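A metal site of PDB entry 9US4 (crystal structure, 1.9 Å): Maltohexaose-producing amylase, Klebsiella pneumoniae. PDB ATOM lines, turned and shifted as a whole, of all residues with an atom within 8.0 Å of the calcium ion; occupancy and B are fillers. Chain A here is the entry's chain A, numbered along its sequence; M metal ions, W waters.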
ATOM      1  N   THR A 179     -23.456  -1.990  -1.751  1.00  0.00           N
ATOM      2  CA  THR A 179     -22.693  -3.078  -1.078  1.00  0.00           C
ATOM      3  C   THR A 179     -23.030  -3.111   0.419  1.00  0.00           C
ATOM      4  O   THR A 179     -23.198  -4.218   0.955  1.00  0.00           O
ATOM      5  CB  THR A 179     -21.187  -2.920  -1.331  1.00  0.00           C
ATOM      6  OG1 THR A 179     -20.989  -2.929  -2.742  1.00  0.00           O
ATOM      7  CG2 THR A 179     -20.366  -4.022  -0.690  1.00  0.00           C
ATOM      8  N   ASP A 180     -23.150  -1.944   1.058  1.00  0.00           N
ATOM      9  CA  ASP A 180     -23.400  -1.829   2.516  1.00  0.00           C
ATOM     10  C   ASP A 180     -24.739  -2.490   2.886  1.00  0.00           C
ATOM     11  O   ASP A 180     -24.875  -2.914   4.056  1.00  0.00           O
ATOM     12  CB  ASP A 180     -23.398  -0.384   2.992  1.00  0.00           C
ATOM     13  CG  ASP A 180     -23.676  -0.283   4.482  1.00  0.00           C
ATOM     14  OD1 ASP A 180     -22.828  -0.754   5.263  1.00  0.00           O
ATOM     15  OD2 ASP A 180     -24.756   0.204   4.843  1.00  0.00           O
ATOM     16  N   VAL A 183     -24.962  -7.907   1.643  1.00  0.00           N
ATOM     17  CA  VAL A 183     -24.510  -9.050   2.498  1.00  0.00           C
ATOM     18  C   VAL A 183     -23.334  -8.610   3.366  1.00  0.00           C
ATOM     19  O   VAL A 183     -22.290  -8.200   2.815  1.00  0.00           O
ATOM     20  CB  VAL A 183     -24.147 -10.287   1.650  1.00  0.00           C
ATOM     21  CG1 VAL A 183     -23.662 -11.438   2.516  1.00  0.00           C
ATOM     22  CG2 VAL A 183     -25.296 -10.735   0.770  1.00  0.00           C
ATOM     23  N   ASN A 184     -23.502  -8.712   4.690  1.00  0.00           N
ATOM     24  CA  ASN A 184     -22.424  -8.521   5.698  1.00  0.00           C
ATOM     25  C   ASN A 184     -21.652  -9.843   5.825  1.00  0.00           C
ATOM     26  O   ASN A 184     -22.102 -10.723   6.569  1.00  0.00           O
ATOM     27  CB  ASN A 184     -23.017  -8.049   7.033  1.00  0.00           C
ATOM     28  CG  ASN A 184     -21.967  -7.623   8.034  1.00  0.00           C
ATOM     29  OD1 ASN A 184     -20.771  -7.834   7.829  1.00  0.00           O
ATOM     30  ND2 ASN A 184     -22.402  -7.006   9.122  1.00  0.00           N
ATOM     31  N   GLY A 185     -20.546  -9.974   5.085  1.00  0.00           N
ATOM     32  CA  GLY A 185     -19.658 -11.139   5.119  1.00  0.00           C
ATOM     33  C   GLY A 185     -18.828 -11.191   6.404  1.00  0.00           C
ATOM     34  O   GLY A 185     -18.544 -12.306   6.864  1.00  0.00           O
ATOM     35  N   ASN A 186     -18.440 -10.032   6.935  1.00  0.00           N
ATOM     36  CA  ASN A 186     -17.581  -9.913   8.158  1.00  0.00           C
ATOM     37  C   ASN A 186     -18.073  -8.758   9.020  1.00  0.00           C
ATOM     38  O   ASN A 186     -17.907  -7.598   8.655  1.00  0.00           O
ATOM     39  CB  ASN A 186     -16.106  -9.736   7.787  1.00  0.00           C
ATOM     40  CG  ASN A 186     -15.185  -9.844   8.987  1.00  0.00           C
ATOM     41  OD1 ASN A 186     -15.645  -9.893  10.127  1.00  0.00           O
ATOM     42  ND2 ASN A 186     -13.883  -9.879   8.739  1.00  0.00           N
ATOM     43  N   PRO A 187     -18.676  -9.031  10.199  1.00  0.00           N
ATOM     44  CA  PRO A 187     -19.160  -7.962  11.073  1.00  0.00           C
ATOM     45  C   PRO A 187     -18.040  -7.111  11.703  1.00  0.00           C
ATOM     46  O   PRO A 187     -18.347  -6.042  12.206  1.00  0.00           O
ATOM     47  CB  PRO A 187     -19.941  -8.675  12.187  1.00  0.00           C
ATOM     48  CG  PRO A 187     -20.097 -10.117  11.717  1.00  0.00           C
ATOM     49  CD  PRO A 187     -18.962 -10.363  10.750  1.00  0.00           C
ATOM     50  N   ALA A 188     -16.796  -7.596  11.671  1.00  0.00           N
ATOM     51  CA  ALA A 188     -15.609  -6.980  12.322  1.00  0.00           C
ATOM     52  C   ALA A 188     -15.324  -5.591  11.739  1.00  0.00           C
ATOM     53  O   ALA A 188     -14.773  -4.759  12.475  1.00  0.00           O
ATOM     54  CB  ALA A 188     -14.415  -7.886  12.188  1.00  0.00           C
ATOM     55  N   ASN A 189     -15.660  -5.359  10.462  1.00  0.00           N
ATOM     56  CA  ASN A 189     -15.305  -4.102   9.743  1.00  0.00           C
ATOM     57  C   ASN A 189     -16.514  -3.155   9.658  1.00  0.00           C
ATOM     58  O   ASN A 189     -16.378  -2.121   8.981  1.00  0.00           O
ATOM     59  CB  ASN A 189     -14.718  -4.418   8.355  1.00  0.00           C
ATOM     60  CG  ASN A 189     -15.649  -5.245   7.487  1.00  0.00           C
ATOM     61  OD1 ASN A 189     -16.874  -5.174   7.636  1.00  0.00           O
ATOM     62  ND2 ASN A 189     -15.081  -6.018   6.575  1.00  0.00           N
ATOM     63  N   ASP A 190     -17.608  -3.454  10.352  1.00  0.00           N
ATOM     64  CA  ASP A 190     -18.887  -2.690  10.280  1.00  0.00           C
ATOM     65  C   ASP A 190     -18.720  -1.265  10.840  1.00  0.00           C
ATOM     66  O   ASP A 190     -19.483  -0.380  10.387  1.00  0.00           O
ATOM     67  CB  ASP A 190     -20.018  -3.400  11.038  1.00  0.00           C
ATOM     68  CG  ASP A 190     -20.444  -4.711  10.394  1.00  0.00           C
ATOM     69  OD1 ASP A 190     -19.883  -5.056   9.337  1.00  0.00           O
ATOM     70  OD2 ASP A 190     -21.323  -5.380  10.969  1.00  0.00           O
ATOM     71  N   ASN A 191     -17.794  -1.054  11.770  1.00  0.00           N
ATOM     72  CA  ASN A 191     -17.652   0.210  12.541  1.00  0.00           C
ATOM     73  C   ASN A 191     -16.244   0.787  12.323  1.00  0.00           C
ATOM     74  O   ASN A 191     -15.646   1.272  13.306  1.00  0.00           O
ATOM     75  CB  ASN A 191     -17.986  -0.020  14.014  1.00  0.00           C
ATOM     76  CG  ASN A 191     -19.395  -0.554  14.200  1.00  0.00           C
ATOM     77  OD1 ASN A 191     -20.364   0.204  14.106  1.00  0.00           O
ATOM     78  ND2 ASN A 191     -19.524  -1.846  14.437  1.00  0.00           N
ATOM     79  N   SER A 192     -15.757   0.760  11.085  1.00  0.00           N
ATOM     80  CA  SER A 192     -14.426   1.309  10.688  1.00  0.00           C
ATOM     81  C   SER A 192     -14.377   2.806  11.023  1.00  0.00           C
ATOM     82  O   SER A 192     -15.431   3.482  10.906  1.00  0.00           O
ATOM     83  CB  SER A 192     -14.136   1.066   9.232  1.00  0.00           C
ATOM     84  OG  SER A 192     -14.173  -0.319   8.914  1.00  0.00           O
ATOM     85  N   PHE A 206     -23.890   2.784   8.220  1.00  0.00           N
ATOM     86  CA  PHE A 206     -23.304   1.571   7.606  1.00  0.00           C
ATOM     87  C   PHE A 206     -23.944   0.350   8.283  1.00  0.00           C
ATOM     88  O   PHE A 206     -23.646   0.107   9.459  1.00  0.00           O
ATOM     89  CB  PHE A 206     -21.773   1.563   7.755  1.00  0.00           C
ATOM     90  CG  PHE A 206     -21.028   2.464   6.813  1.00  0.00           C
ATOM     91  CD1 PHE A 206     -20.805   3.803   7.114  1.00  0.00           C
ATOM     92  CD2 PHE A 206     -20.505   1.975   5.622  1.00  0.00           C
ATOM     93  CE1 PHE A 206     -20.099   4.624   6.251  1.00  0.00           C
ATOM     94  CE2 PHE A 206     -19.786   2.797   4.764  1.00  0.00           C
ATOM     95  CZ  PHE A 206     -19.597   4.122   5.074  1.00  0.00           C
ATOM     96  N   HIS A 207     -24.815  -0.362   7.567  1.00  0.00           N
ATOM     97  CA  HIS A 207     -25.442  -1.642   8.023  1.00  0.00           C
ATOM     98  C   HIS A 207     -24.372  -2.737   8.160  1.00  0.00           C
ATOM     99  O   HIS A 207     -24.558  -3.619   9.025  1.00  0.00           O
ATOM    100  CB  HIS A 207     -26.573  -2.053   7.077  1.00  0.00           C
ATOM    101  CG  HIS A 207     -27.791  -1.202   7.190  1.00  0.00           C
ATOM    102  ND1 HIS A 207     -29.040  -1.647   6.818  1.00  0.00           N
ATOM    103  CD2 HIS A 207     -27.949   0.063   7.635  1.00  0.00           C
ATOM    104  CE1 HIS A 207     -29.924  -0.693   7.016  1.00  0.00           C
ATOM    105  NE2 HIS A 207     -29.277   0.370   7.515  1.00  0.00           N
ATOM    106  N   GLY A 208     -23.321  -2.680   7.339  1.00  0.00           N
ATOM    107  CA  GLY A 208     -22.152  -3.585   7.452  1.00  0.00           C
ATOM    108  C   GLY A 208     -21.978  -4.498   6.250  1.00  0.00           C
ATOM    109  O   GLY A 208     -21.095  -5.382   6.321  1.00  0.00           O
ATOM    110  N   GLY A 209     -22.746  -4.312   5.174  1.00  0.00           N
ATOM    111  CA  GLY A 209     -22.527  -5.040   3.907  1.00  0.00           C
ATOM    112  C   GLY A 209     -21.146  -4.757   3.353  1.00  0.00           C
ATOM    113  O   GLY A 209     -20.680  -3.603   3.475  1.00  0.00           O
ATOM    114  N   ASP A 210     -20.480  -5.775   2.783  1.00  0.00           N
ATOM    115  CA  ASP A 210     -19.058  -5.659   2.369  1.00  0.00           C
ATOM    116  C   ASP A 210     -18.791  -6.495   1.108  1.00  0.00           C
ATOM    117  O   ASP A 210     -19.709  -7.228   0.674  1.00  0.00           O
ATOM    118  CB  ASP A 210     -18.132  -6.021   3.534  1.00  0.00           C
ATOM    119  CG  ASP A 210     -18.518  -7.306   4.252  1.00  0.00           C
ATOM    120  OD1 ASP A 210     -18.803  -8.314   3.560  1.00  0.00           O
ATOM    121  OD2 ASP A 210     -18.526  -7.303   5.500  1.00  0.00           O
ATOM    122  N   LEU A 211     -17.594  -6.364   0.546  1.00  0.00           N
ATOM    123  CA  LEU A 211     -17.181  -6.982  -0.742  1.00  0.00           C
ATOM    124  C   LEU A 211     -17.171  -8.507  -0.596  1.00  0.00           C
ATOM    125  O   LEU A 211     -17.580  -9.188  -1.553  1.00  0.00           O
ATOM    126  CB  LEU A 211     -15.814  -6.448  -1.158  1.00  0.00           C
ATOM    127  CG  LEU A 211     -15.749  -4.942  -1.448  1.00  0.00           C
ATOM    128  CD1 LEU A 211     -14.330  -4.518  -1.750  1.00  0.00           C
ATOM    129  CD2 LEU A 211     -16.682  -4.566  -2.593  1.00  0.00           C
ATOM    130  N   GLN A 212     -16.731  -9.014   0.565  1.00  0.00           N
ATOM    131  CA  GLN A 212     -16.753 -10.466   0.904  1.00  0.00           C
ATOM    132  C   GLN A 212     -18.185 -10.998   0.771  1.00  0.00           C
ATOM    133  O   GLN A 212     -18.375 -12.024   0.104  1.00  0.00           O
ATOM    134  CB  GLN A 212     -16.235 -10.699   2.323  1.00  0.00           C
ATOM    135  CG  GLN A 212     -16.306 -12.166   2.750  1.00  0.00           C
ATOM    136  CD  GLN A 212     -15.882 -12.383   4.178  1.00  0.00           C
ATOM    137  OE1 GLN A 212     -15.559 -11.454   4.904  1.00  0.00           O
ATOM    138  NE2 GLN A 212     -15.860 -13.639   4.579  1.00  0.00           N
ATOM    139  N   GLY A 213     -19.150 -10.323   1.404  1.00  0.00           N
ATOM    140  CA  GLY A 213     -20.569 -10.724   1.386  1.00  0.00           C
ATOM    141  C   GLY A 213     -21.113 -10.774  -0.028  1.00  0.00           C
ATOM    142  O   GLY A 213     -21.811 -11.748  -0.362  1.00  0.00           O
ATOM    143  N   ALA A 268     -12.468   0.877   4.599  1.00  0.00           N
ATOM    144  CA  ALA A 268     -12.204  -0.284   5.489  1.00  0.00           C
ATOM    145  C   ALA A 268     -13.497  -1.077   5.746  1.00  0.00           C
ATOM    146  O   ALA A 268     -13.401  -2.288   5.994  1.00  0.00           O
ATOM    147  CB  ALA A 268     -11.589   0.192   6.787  1.00  0.00           C
ATOM    148  N   ASN A 269     -14.665  -0.421   5.671  1.00  0.00           N
ATOM    149  CA  ASN A 269     -15.989  -1.089   5.801  1.00  0.00           C
ATOM    150  C   ASN A 269     -16.186  -2.102   4.672  1.00  0.00           C
ATOM    151  O   ASN A 269     -16.836  -3.128   4.910  1.00  0.00           O
ATOM    152  CB  ASN A 269     -17.162  -0.103   5.827  1.00  0.00           C
ATOM    153  CG  ASN A 269     -17.657   0.189   7.227  1.00  0.00           C
ATOM    154  OD1 ASN A 269     -16.961   0.832   8.004  1.00  0.00           O
ATOM    155  ND2 ASN A 269     -18.851  -0.290   7.549  1.00  0.00           N
ATOM    156  N   MET A 270     -15.658  -1.792   3.476  1.00  0.00           N
ATOM    157  CA  MET A 270     -15.885  -2.589   2.243  1.00  0.00           C
ATOM    158  C   MET A 270     -14.964  -3.818   2.246  1.00  0.00           C
ATOM    159  O   MET A 270     -15.401  -4.879   1.773  1.00  0.00           O
ATOM    160  CB  MET A 270     -15.655  -1.733   0.999  1.00  0.00           C
ATOM    161  CG  MET A 270     -16.706  -0.653   0.848  1.00  0.00           C
ATOM    162  SD  MET A 270     -18.311  -1.387   0.475  1.00  0.00           S
ATOM    163  CE  MET A 270     -19.377  -0.460   1.577  1.00  0.00           C
ATOM    164  N   GLY A 271     -13.751  -3.667   2.791  1.00  0.00           N
ATOM    165  CA  GLY A 271     -12.810  -4.776   3.029  1.00  0.00           C
ATOM    166  C   GLY A 271     -11.409  -4.453   2.547  1.00  0.00           C
ATOM    167  O   GLY A 271     -11.061  -3.249   2.465  1.00  0.00           O
HETATM  168 CA    CA M   1     -19.077  -6.003   7.336  1.00  0.00          CA
HETATM  169  O   HOH W   1     -18.851  -3.646   6.589  1.00  0.00           O
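O of Asp 190 lies within hydrogen-bond range of ND2 of Asn 269 (2.9 Å). N of Ala 188 lies within hydrogen-bond range of OD1 of Asn 186 (3.0 Å). The backbone NH of Gly 185 sits at hydrogen-bond distance from the side-chain carboxylate of Asp 210 (2.8 Å). O of Asn 189 sits close to OD1 of Asn 269 (3.2 Å). The backbone NH (N) of Asp 210 lies within hydrogen-bond range of the backbone carbonyl oxygen (O) of Val 183, 3.0 Å away. The backbone NH of Gly 208 lies within hydrogen-bond range of the side-chain carboxylate of Asp 180, at 2.9 Å. The backbone NH of Gly 213 is in hydrogen-bond range of the side-chain carboxylate of Asp 210 (3.0 Å). The side-chain hydroxyl (OG) of Ser 192 lies within hydrogen-bond range of the backbone carbonyl oxygen (O) of Asn 189.
The calcium ion is bound by OD2 of Asp 210 (2.3 Å), O of Gly 208 (2.3 Å), OD1 of Asp 190 (2.4 Å), OD1 of Asn 189 (2.4 Å), O of Asn 186 (2.4 Å), water W1 (2.5 Å) and OD1 of Asn 184 (2.5 Å).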
